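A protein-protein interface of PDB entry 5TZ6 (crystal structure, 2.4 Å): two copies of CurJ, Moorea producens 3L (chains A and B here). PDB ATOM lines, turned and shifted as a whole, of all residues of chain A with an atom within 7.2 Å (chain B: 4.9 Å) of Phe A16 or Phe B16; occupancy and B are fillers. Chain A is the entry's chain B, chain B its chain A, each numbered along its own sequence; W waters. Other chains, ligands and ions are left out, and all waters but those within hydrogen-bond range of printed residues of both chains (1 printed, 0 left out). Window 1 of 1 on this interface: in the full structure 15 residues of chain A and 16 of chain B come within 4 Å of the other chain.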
ATOM      1  N   LEU A   8     -16.213  12.093  25.608  1.00  0.00           N
ATOM      2  CA  LEU A   8     -15.352  12.908  26.460  1.00  0.00           C
ATOM      3  C   LEU A   8     -14.705  12.082  27.564  1.00  0.00           C
ATOM      4  O   LEU A   8     -13.559  12.341  27.949  1.00  0.00           O
ATOM      5  CB  LEU A   8     -16.161  14.054  27.064  1.00  0.00           C
ATOM      6  CG  LEU A   8     -16.925  14.919  26.062  1.00  0.00           C
ATOM      7  CD1 LEU A   8     -17.722  15.996  26.779  1.00  0.00           C
ATOM      8  CD2 LEU A   8     -15.977  15.527  25.041  1.00  0.00           C
ATOM      9  N   GLN A  14     -21.356  13.715  26.541  1.00  0.00           N
ATOM     10  CA  GLN A  14     -21.277  15.102  26.111  1.00  0.00           C
ATOM     11  C   GLN A  14     -21.300  16.039  27.311  1.00  0.00           C
ATOM     12  O   GLN A  14     -21.769  15.688  28.392  1.00  0.00           O
ATOM     13  CB  GLN A  14     -22.422  15.436  25.144  1.00  0.00           C
ATOM     14  CG  GLN A  14     -23.783  15.569  25.808  1.00  0.00           C
ATOM     15  CD  GLN A  14     -24.881  15.942  24.827  1.00  0.00           C
ATOM     16  OE1 GLN A  14     -25.576  16.945  25.001  1.00  0.00           O
ATOM     17  NE2 GLN A  14     -25.049  15.124  23.792  1.00  0.00           N
ATOM     18  N   LYS A  15     -20.743  17.231  27.114  1.00  0.00           N
ATOM     19  CA  LYS A  15     -20.820  18.321  28.076  1.00  0.00           C
ATOM     20  C   LYS A  15     -21.515  19.505  27.423  1.00  0.00           C
ATOM     21  O   LYS A  15     -21.306  19.779  26.238  1.00  0.00           O
ATOM     22  CB  LYS A  15     -19.438  18.749  28.578  1.00  0.00           C
ATOM     23  CG  LYS A  15     -19.401  20.193  29.059  1.00  0.00           C
ATOM     24  CD  LYS A  15     -18.079  20.557  29.713  1.00  0.00           C
ATOM     25  CE  LYS A  15     -18.138  21.963  30.302  1.00  0.00           C
ATOM     26  NZ  LYS A  15     -16.856  22.384  30.937  1.00  0.00           N
ATOM     27  N   PHE A  16     -22.341  20.207  28.189  1.00  0.00           N
ATOM     28  CA  PHE A  16     -23.042  21.364  27.660  1.00  0.00           C
ATOM     29  C   PHE A  16     -23.022  22.515  28.653  1.00  0.00           C
ATOM     30  O   PHE A  16     -23.314  22.328  29.838  1.00  0.00           O
ATOM     31  CB  PHE A  16     -24.492  21.030  27.309  1.00  0.00           C
ATOM     32  CG  PHE A  16     -25.237  22.196  26.750  1.00  0.00           C
ATOM     33  CD1 PHE A  16     -25.029  22.601  25.443  1.00  0.00           C
ATOM     34  CD2 PHE A  16     -26.114  22.914  27.541  1.00  0.00           C
ATOM     35  CE1 PHE A  16     -25.699  23.686  24.925  1.00  0.00           C
ATOM     36  CE2 PHE A  16     -26.788  24.005  27.027  1.00  0.00           C
ATOM     37  CZ  PHE A  16     -26.577  24.392  25.716  1.00  0.00           C
ATOM     38  N   GLN A  17     -22.693  23.706  28.157  1.00  0.00           N
ATOM     39  CA  GLN A  17     -22.889  24.933  28.909  1.00  0.00           C
ATOM     40  C   GLN A  17     -23.174  26.057  27.925  1.00  0.00           C
ATOM     41  O   GLN A  17     -22.888  25.946  26.732  1.00  0.00           O
ATOM     42  CB  GLN A  17     -21.682  25.258  29.796  1.00  0.00           C
ATOM     43  CG  GLN A  17     -20.401  25.540  29.048  1.00  0.00           C
ATOM     44  CD  GLN A  17     -19.240  25.770  29.991  1.00  0.00           C
ATOM     45  OE1 GLN A  17     -18.277  25.004  30.009  1.00  0.00           O
ATOM     46  NE2 GLN A  17     -19.338  26.818  30.802  1.00  0.00           N
ATOM     47  N   SER A  18     -23.761  27.141  28.440  1.00  0.00           N
ATOM     48  CA  SER A  18     -24.234  28.234  27.602  1.00  0.00           C
ATOM     49  C   SER A  18     -24.212  29.547  28.371  1.00  0.00           C
ATOM     50  O   SER A  18     -24.563  29.569  29.559  1.00  0.00           O
ATOM     51  CB  SER A  18     -25.654  27.964  27.089  1.00  0.00           C
ATOM     52  OG  SER A  18     -26.165  29.083  26.383  1.00  0.00           O
ATOM     53  N   PRO A  19     -23.842  30.648  27.724  1.00  0.00           N
ATOM     54  CA  PRO A  19     -23.944  31.958  28.381  1.00  0.00           C
ATOM     55  C   PRO A  19     -25.343  32.244  28.907  1.00  0.00           C
ATOM     56  O   PRO A  19     -25.519  33.100  29.780  1.00  0.00           O
ATOM     57  CB  PRO A  19     -23.549  32.936  27.269  1.00  0.00           C
ATOM     58  CG  PRO A  19     -22.707  32.129  26.345  1.00  0.00           C
ATOM     59  CD  PRO A  19     -23.263  30.743  26.376  1.00  0.00           C
ATOM     60  N   SER A  21     -27.259  29.890  30.334  1.00  0.00           N
ATOM     61  CA  SER A  21     -27.561  28.871  31.329  1.00  0.00           C
ATOM     62  C   SER A  21     -26.522  28.978  32.433  1.00  0.00           C
ATOM     63  O   SER A  21     -25.319  28.953  32.155  1.00  0.00           O
ATOM     64  CB  SER A  21     -27.550  27.467  30.712  1.00  0.00           C
ATOM     65  OG  SER A  21     -27.886  26.482  31.670  1.00  0.00           O
ATOM     66  N   GLU A  23     -26.158  26.731  34.823  1.00  0.00           N
ATOM     67  CA  GLU A  23     -25.705  25.397  35.172  1.00  0.00           C
ATOM     68  C   GLU A  23     -24.773  24.845  34.104  1.00  0.00           C
ATOM     69  O   GLU A  23     -24.799  25.255  32.945  1.00  0.00           O
ATOM     70  CB  GLU A  23     -26.893  24.448  35.346  1.00  0.00           C
ATOM     71  CG  GLU A  23     -27.809  24.780  36.509  1.00  0.00           C
ATOM     72  CD  GLU A  23     -28.962  25.676  36.099  1.00  0.00           C
ATOM     73  OE1 GLU A  23     -29.053  26.015  34.898  1.00  0.00           O
ATOM     74  OE2 GLU A  23     -29.781  26.036  36.973  1.00  0.00           O
ATOM     75  N   ILE A  24     -23.943  23.898  34.519  1.00  0.00           N
ATOM     76  CA  ILE A  24     -23.138  23.094  33.612  1.00  0.00           C
ATOM     77  C   ILE A  24     -23.722  21.691  33.609  1.00  0.00           C
ATOM     78  O   ILE A  24     -24.037  21.138  34.668  1.00  0.00           O
ATOM     79  CB  ILE A  24     -21.653  23.080  34.025  1.00  0.00           C
ATOM     80  CG1 ILE A  24     -21.083  24.498  34.029  1.00  0.00           C
ATOM     81  CG2 ILE A  24     -20.842  22.174  33.110  1.00  0.00           C
ATOM     82  CD1 ILE A  24     -19.625  24.556  34.430  1.00  0.00           C
ATOM     83  N   PHE A  25     -23.862  21.114  32.424  1.00  0.00           N
ATOM     84  CA  PHE A  25     -24.512  19.824  32.271  1.00  0.00           C
ATOM     85  C   PHE A  25     -23.526  18.815  31.712  1.00  0.00           C
ATOM     86  O   PHE A  25     -22.744  19.132  30.814  1.00  0.00           O
ATOM     87  CB  PHE A  25     -25.725  19.916  31.347  1.00  0.00           C
ATOM     88  CG  PHE A  25     -26.818  20.797  31.870  1.00  0.00           C
ATOM     89  CD1 PHE A  25     -26.834  22.149  31.580  1.00  0.00           C
ATOM     90  CD2 PHE A  25     -27.834  20.270  32.645  1.00  0.00           C
ATOM     91  CE1 PHE A  25     -27.842  22.960  32.057  1.00  0.00           C
ATOM     92  CE2 PHE A  25     -28.846  21.075  33.126  1.00  0.00           C
ATOM     93  CZ  PHE A  25     -28.851  22.422  32.832  1.00  0.00           C
ATOM     94  N   PHE A  26     -23.570  17.603  32.247  1.00  0.00           N
ATOM     95  CA  PHE A  26     -22.872  16.471  31.666  1.00  0.00           C
ATOM     96  C   PHE A  26     -23.885  15.377  31.377  1.00  0.00           C
ATOM     97  O   PHE A  26     -24.765  15.098  32.198  1.00  0.00           O
ATOM     98  CB  PHE A  26     -21.784  15.967  32.604  1.00  0.00           C
ATOM     99  CG  PHE A  26     -20.761  17.008  32.935  1.00  0.00           C
ATOM    100  CD1 PHE A  26     -20.960  17.873  33.997  1.00  0.00           C
ATOM    101  CD2 PHE A  26     -19.617  17.142  32.173  1.00  0.00           C
ATOM    102  CE1 PHE A  26     -20.024  18.842  34.304  1.00  0.00           C
ATOM    103  CE2 PHE A  26     -18.679  18.108  32.476  1.00  0.00           C
ATOM    104  CZ  PHE A  26     -18.884  18.960  33.543  1.00  0.00           C
ATOM    105  N   GLU A  27     -23.757  14.756  30.213  1.00  0.00           N
ATOM    106  CA  GLU A  27     -24.748  13.806  29.744  1.00  0.00           C
ATOM    107  C   GLU A  27     -24.064  12.505  29.370  1.00  0.00           C
ATOM    108  O   GLU A  27     -23.007  12.499  28.722  1.00  0.00           O
ATOM    109  CB  GLU A  27     -25.535  14.357  28.552  1.00  0.00           C
ATOM    110  CG  GLU A  27     -26.701  13.476  28.149  1.00  0.00           C
ATOM    111  CD  GLU A  27     -27.595  14.128  27.116  1.00  0.00           C
ATOM    112  OE1 GLU A  27     -28.501  14.891  27.516  1.00  0.00           O
ATOM    113  OE2 GLU A  27     -27.392  13.877  25.908  1.00  0.00           O
ATOM    114  N   TYR A  29     -24.953   7.997  28.788  1.00  0.00           N
ATOM    115  CA  TYR A  29     -25.953   7.011  28.376  1.00  0.00           C
ATOM    116  C   TYR A  29     -25.652   5.679  29.056  1.00  0.00           C
ATOM    117  O   TYR A  29     -24.719   4.969  28.669  1.00  0.00           O
ATOM    118  CB  TYR A  29     -25.986   6.893  26.855  1.00  0.00           C
ATOM    119  CG  TYR A  29     -26.281   8.224  26.202  1.00  0.00           C
ATOM    120  CD1 TYR A  29     -27.522   8.828  26.350  1.00  0.00           C
ATOM    121  CD2 TYR A  29     -25.304   8.901  25.484  1.00  0.00           C
ATOM    122  CE1 TYR A  29     -27.792  10.054  25.777  1.00  0.00           C
ATOM    123  CE2 TYR A  29     -25.566  10.129  24.910  1.00  0.00           C
ATOM    124  CZ  TYR A  29     -26.810  10.699  25.059  1.00  0.00           C
ATOM    125  OH  TYR A  29     -27.078  11.921  24.491  1.00  0.00           O
ATOM    126  N   THR A  91     -30.790   7.808  30.216  1.00  0.00           N
ATOM    127  CA  THR A  91     -29.998   9.021  30.139  1.00  0.00           C
ATOM    128  C   THR A  91     -29.718   9.516  31.550  1.00  0.00           C
ATOM    129  O   THR A  91     -30.640   9.688  32.353  1.00  0.00           O
ATOM    130  CB  THR A  91     -30.737  10.090  29.340  1.00  0.00           C
ATOM    131  OG1 THR A  91     -30.967   9.614  28.010  1.00  0.00           O
ATOM    132  CG2 THR A  91     -29.922  11.371  29.282  1.00  0.00           C
ATOM    133  N   GLN A  93     -27.718  12.552  33.745  1.00  0.00           N
ATOM    134  CA  GLN A  93     -27.144  13.883  33.658  1.00  0.00           C
ATOM    135  C   GLN A  93     -26.618  14.306  35.017  1.00  0.00           C
ATOM    136  O   GLN A  93     -27.239  14.035  36.051  1.00  0.00           O
ATOM    137  CB  GLN A  93     -28.167  14.910  33.162  1.00  0.00           C
ATOM    138  CG  GLN A  93     -28.634  14.692  31.733  1.00  0.00           C
ATOM    139  CD  GLN A  93     -29.705  15.682  31.325  1.00  0.00           C
ATOM    140  OE1 GLN A  93     -30.417  16.223  32.174  1.00  0.00           O
ATOM    141  NE2 GLN A  93     -29.821  15.932  30.022  1.00  0.00           N
ATOM    142  N   VAL A  94     -25.461  14.953  35.001  1.00  0.00           N
ATOM    143  CA  VAL A  94     -24.946  15.677  36.152  1.00  0.00           C
ATOM    144  C   VAL A  94     -25.222  17.152  35.917  1.00  0.00           C
ATOM    145  O   VAL A  94     -24.870  17.699  34.863  1.00  0.00           O
ATOM    146  CB  VAL A  94     -23.444  15.418  36.357  1.00  0.00           C
ATOM    147  CG1 VAL A  94     -22.932  16.218  37.546  1.00  0.00           C
ATOM    148  CG2 VAL A  94     -23.183  13.931  36.551  1.00  0.00           C
ATOM    149  N   VAL A  95     -25.866  17.792  36.887  1.00  0.00           N
ATOM    150  CA  VAL A  95     -26.238  19.196  36.790  1.00  0.00           C
ATOM    151  C   VAL A  95     -25.501  19.943  37.890  1.00  0.00           C
ATOM    152  O   VAL A  95     -25.675  19.639  39.079  1.00  0.00           O
ATOM    153  CB  VAL A  95     -27.755  19.397  36.904  1.00  0.00           C
ATOM    154  CG1 VAL A  95     -28.113  20.845  36.596  1.00  0.00           C
ATOM    155  CG2 VAL A  95     -28.480  18.437  35.973  1.00  0.00           C
ATOM    156  N   PHE A 110     -33.315   9.546  33.461  1.00  0.00           N
ATOM    157  CA  PHE A 110     -34.637   9.438  32.856  1.00  0.00           C
ATOM    158  C   PHE A 110     -34.504   8.596  31.595  1.00  0.00           C
ATOM    159  O   PHE A 110     -33.420   8.492  31.019  1.00  0.00           O
ATOM    160  CB  PHE A 110     -35.229  10.817  32.537  1.00  0.00           C
ATOM    161  CG  PHE A 110     -34.314  11.702  31.731  1.00  0.00           C
ATOM    162  CD1 PHE A 110     -33.466  12.598  32.360  1.00  0.00           C
ATOM    163  CD2 PHE A 110     -34.309  11.644  30.348  1.00  0.00           C
ATOM    164  CE1 PHE A 110     -32.629  13.416  31.626  1.00  0.00           C
ATOM    165  CE2 PHE A 110     -33.473  12.459  29.609  1.00  0.00           C
ATOM    166  CZ  PHE A 110     -32.632  13.347  30.249  1.00  0.00           C
ATOM    167  N   GLN B  14     -25.689  19.158  17.938  1.00  0.00           N
ATOM    168  CA  GLN B  14     -26.329  18.430  19.026  1.00  0.00           C
ATOM    169  C   GLN B  14     -27.487  19.238  19.585  1.00  0.00           C
ATOM    170  O   GLN B  14     -27.552  20.458  19.442  1.00  0.00           O
ATOM    171  CB  GLN B  14     -25.358  18.068  20.159  1.00  0.00           C
ATOM    172  CG  GLN B  14     -24.971  19.217  21.067  1.00  0.00           C
ATOM    173  CD  GLN B  14     -24.098  18.766  22.226  1.00  0.00           C
ATOM    174  OE1 GLN B  14     -24.425  19.000  23.391  1.00  0.00           O
ATOM    175  NE2 GLN B  14     -22.990  18.102  21.910  1.00  0.00           N
ATOM    176  N   LYS B  15     -28.414  18.524  20.212  1.00  0.00           N
ATOM    177  CA  LYS B  15     -29.531  19.107  20.938  1.00  0.00           C
ATOM    178  C   LYS B  15     -29.422  18.709  22.402  1.00  0.00           C
ATOM    179  O   LYS B  15     -29.045  17.577  22.719  1.00  0.00           O
ATOM    180  CB  LYS B  15     -30.865  18.626  20.355  1.00  0.00           C
ATOM    181  CG  LYS B  15     -32.021  18.625  21.336  1.00  0.00           C
ATOM    182  CD  LYS B  15     -33.324  18.267  20.638  1.00  0.00           C
ATOM    183  CE  LYS B  15     -34.514  18.385  21.584  1.00  0.00           C
ATOM    184  NZ  LYS B  15     -35.792  17.999  20.924  1.00  0.00           N
ATOM    185  N   PHE B  16     -29.744  19.641  23.294  1.00  0.00           N
ATOM    186  CA  PHE B  16     -29.696  19.360  24.720  1.00  0.00           C
ATOM    187  C   PHE B  16     -30.928  19.915  25.411  1.00  0.00           C
ATOM    188  O   PHE B  16     -31.295  21.077  25.205  1.00  0.00           O
ATOM    189  CB  PHE B  16     -28.448  19.946  25.382  1.00  0.00           C
ATOM    190  CG  PHE B  16     -28.367  19.638  26.845  1.00  0.00           C
ATOM    191  CD1 PHE B  16     -27.968  18.387  27.280  1.00  0.00           C
ATOM    192  CD2 PHE B  16     -28.744  20.581  27.784  1.00  0.00           C
ATOM    193  CE1 PHE B  16     -27.913  18.088  28.630  1.00  0.00           C
ATOM    194  CE2 PHE B  16     -28.693  20.292  29.134  1.00  0.00           C
ATOM    195  CZ  PHE B  16     -28.278  19.042  29.559  1.00  0.00           C
ATOM    196  N   GLN B  17     -31.542  19.080  26.244  1.00  0.00           N
ATOM    197  CA  GLN B  17     -32.565  19.528  27.171  1.00  0.00           C
ATOM    198  C   GLN B  17     -32.492  18.666  28.419  1.00  0.00           C
ATOM    199  O   GLN B  17     -31.923  17.571  28.409  1.00  0.00           O
ATOM    200  CB  GLN B  17     -33.961  19.493  26.540  1.00  0.00           C
ATOM    201  CG  GLN B  17     -34.449  18.125  26.133  1.00  0.00           C
ATOM    202  CD  GLN B  17     -35.804  18.192  25.462  1.00  0.00           C
ATOM    203  OE1 GLN B  17     -35.940  17.882  24.278  1.00  0.00           O
ATOM    204  NE2 GLN B  17     -36.819  18.599  26.218  1.00  0.00           N
ATOM    205  N   SER B  18     -33.070  19.185  29.505  1.00  0.00           N
ATOM    206  CA  SER B  18     -32.942  18.580  30.821  1.00  0.00           C
ATOM    207  C   SER B  18     -34.162  18.903  31.667  1.00  0.00           C
ATOM    208  O   SER B  18     -34.697  20.019  31.570  1.00  0.00           O
ATOM    209  CB  SER B  18     -31.676  19.069  31.536  1.00  0.00           C
ATOM    210  OG  SER B  18     -31.601  18.569  32.861  1.00  0.00           O
ATOM    211  N   GLU B  23     -35.137  25.992  29.331  1.00  0.00           N
ATOM    212  CA  GLU B  23     -34.831  26.214  27.924  1.00  0.00           C
ATOM    213  C   GLU B  23     -34.415  24.917  27.231  1.00  0.00           C
ATOM    214  O   GLU B  23     -33.929  23.972  27.857  1.00  0.00           O
ATOM    215  CB  GLU B  23     -33.728  27.264  27.757  1.00  0.00           C
ATOM    216  CG  GLU B  23     -34.124  28.666  28.179  1.00  0.00           C
ATOM    217  CD  GLU B  23     -33.771  28.964  29.621  1.00  0.00           C
ATOM    218  OE1 GLU B  23     -33.188  28.084  30.288  1.00  0.00           O
ATOM    219  OE2 GLU B  23     -34.082  30.079  30.088  1.00  0.00           O
ATOM    220  N   ILE B  24     -34.601  24.893  25.914  1.00  0.00           N
ATOM    221  CA  ILE B  24     -34.085  23.843  25.045  1.00  0.00           C
ATOM    222  C   ILE B  24     -32.964  24.441  24.210  1.00  0.00           C
ATOM    223  O   ILE B  24     -33.080  25.566  23.712  1.00  0.00           O
ATOM    224  CB  ILE B  24     -35.185  23.253  24.141  1.00  0.00           C
ATOM    225  CG1 ILE B  24     -36.317  22.670  24.979  1.00  0.00           C
ATOM    226  CG2 ILE B  24     -34.605  22.197  23.212  1.00  0.00           C
ATOM    227  CD1 ILE B  24     -37.432  22.086  24.141  1.00  0.00           C
ATOM    228  N   PHE B  25     -31.875  23.696  24.059  1.00  0.00           N
ATOM    229  CA  PHE B  25     -30.686  24.208  23.396  1.00  0.00           C
ATOM    230  C   PHE B  25     -30.361  23.388  22.158  1.00  0.00           C
ATOM    231  O   PHE B  25     -30.491  22.162  22.160  1.00  0.00           O
ATOM    232  CB  PHE B  25     -29.485  24.202  24.343  1.00  0.00           C
ATOM    233  CG  PHE B  25     -29.656  25.088  25.544  1.00  0.00           C
ATOM    234  CD1 PHE B  25     -30.198  24.590  26.720  1.00  0.00           C
ATOM    235  CD2 PHE B  25     -29.270  26.418  25.500  1.00  0.00           C
ATOM    236  CE1 PHE B  25     -30.356  25.406  27.829  1.00  0.00           C
ATOM    237  CE2 PHE B  25     -29.427  27.240  26.604  1.00  0.00           C
ATOM    238  CZ  PHE B  25     -29.971  26.734  27.770  1.00  0.00           C
ATOM    239  N   GLU B  27     -26.973  23.231  19.404  1.00  0.00           N
ATOM    240  CA  GLU B  27     -25.581  23.642  19.317  1.00  0.00           C
ATOM    241  C   GLU B  27     -24.991  23.204  17.986  1.00  0.00           C
ATOM    242  O   GLU B  27     -25.212  22.073  17.529  1.00  0.00           O
ATOM    243  CB  GLU B  27     -24.747  23.062  20.467  1.00  0.00           C
ATOM    244  CG  GLU B  27     -23.326  23.599  20.515  1.00  0.00           C
ATOM    245  CD  GLU B  27     -22.576  23.165  21.761  1.00  0.00           C
ATOM    246  OE1 GLU B  27     -22.710  23.843  22.802  1.00  0.00           O
ATOM    247  OE2 GLU B  27     -21.849  22.151  21.696  1.00  0.00           O
ATOM    248  N   GLN B  93     -25.525  28.716  19.205  1.00  0.00           N
ATOM    249  CA  GLN B  93     -26.581  28.041  19.938  1.00  0.00           C
ATOM    250  C   GLN B  93     -27.917  28.703  19.642  1.00  0.00           C
ATOM    251  O   GLN B  93     -27.998  29.930  19.492  1.00  0.00           O
ATOM    252  CB  GLN B  93     -26.333  28.059  21.441  1.00  0.00           C
ATOM    253  CG  GLN B  93     -25.122  27.283  21.902  1.00  0.00           C
ATOM    254  CD  GLN B  93     -24.919  27.415  23.397  1.00  0.00           C
ATOM    255  OE1 GLN B  93     -25.362  28.391  24.006  1.00  0.00           O
ATOM    256  NE2 GLN B  93     -24.273  26.425  24.003  1.00  0.00           N
HETATM  257  O   HOH W   1     -21.157  23.429  25.301  1.00  0.00           O
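Of the printed residues of chain B, Pro A19 touches Gln B93.
Of the printed residues of chain B, Phe A25 touches Phe B16 (3.2 Å) and Ser B18 (3.7 Å).
Printed residues of chain B within 4 Å of Gln A93: Phe B16, Gln B17 and Ser B18.
Val A95 touches none of the printed residues of chain B.
Phe B16 touches just these residues of chain A: Gln A14 (3.6 Å), Phe A16 (3.5 Å), Phe A25 (3.2 Å), Glu A27 (3.4 Å) and Gln A93 (3.2 Å).
Printed residues of chain A within 4 Å of Gln B17: Gln A93.
Printed residues of chain A within 4 Å of Glu B27: Phe A16.
Water W1 bridges OE1 of Glu B27 (3.0 Å) and N of Gln A17 (3.3 Å).
Among the printed residues, pairs that only touch across the chains: Phe A16 with Phe B25, Gln A93 with Phe B16, Phe A16 with Gln B93, Phe A25 with Phe B16, Glu A27 with Phe B16, Phe A16 with Phe B16, Gln A14 with Phe B16, Phe A16 with Glu B27, Phe A25 with Ser B18, Ser A18 with Phe B25, Ser A21 with Phe B25 and Pro A19 with Gln B93.
Gln A14 touches Phe B16, but with the chains exchanged Phe A16 does not touch Gln B14 (4.2 Å).
Phe A16 touches its own counterpart, Phe B16.
Phe A16 touches Glu B27, and with the chains exchanged Glu A27 touches Phe B16.
Ser A18 touches Phe B25, and with the chains exchanged Phe A25 touches Ser B18.
Of the 17 pairs that touch across the chains among the printed residues, 14 have their exchanged pair printed and touching as well.
Hydrophobic or aromatic side chains of chain B within 4 Å of the printed part of chain A: Phe B16 and Phe B25.
Among the printed residues, 17 pairs touch across the chains.
OG of Ser B18 is in hydrogen-bond range of OE1 of Gln A93, 2.7 Å away.
O of Gln B17 is in hydrogen-bond range of NE2 of Gln A93 (3.1 Å).
The side-chain amide nitrogen of Gln B93 sits at hydrogen-bond distance from the backbone carbonyl oxygen of Gln A17, 3.1 Å away.
OE1 of Gln B93 lies within hydrogen-bond range of OG of Ser A18 (2.6 Å).
OE1 of Gln A14 sits close to OE1 of Gln B14 (2.9 Å).
The side-chain amino group (NZ) of Lys A15 lies close to the side-chain amide oxygen (OE1) of Gln A17, at 3.1 Å.
OE1 of Glu B27 is in hydrogen-bond range of NE2 of Gln B93 (3.2 Å).
The backbone carbonyl oxygen of Gln B14 lies within hydrogen-bond range of the backbone NH of Glu B27 (2.8 Å).
The backbone NH of Phe A16 sits at hydrogen-bond distance from the backbone carbonyl oxygen of Phe A25.
The side-chain amino group (NZ) of Lys B15 sits close to the side-chain amide oxygen (OE1) of Gln B17, at 3.4 Å.
The side-chain carboxylate (OE2) of Glu A27 is in hydrogen-bond range of the side-chain hydroxyl (OH) of Tyr A29.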
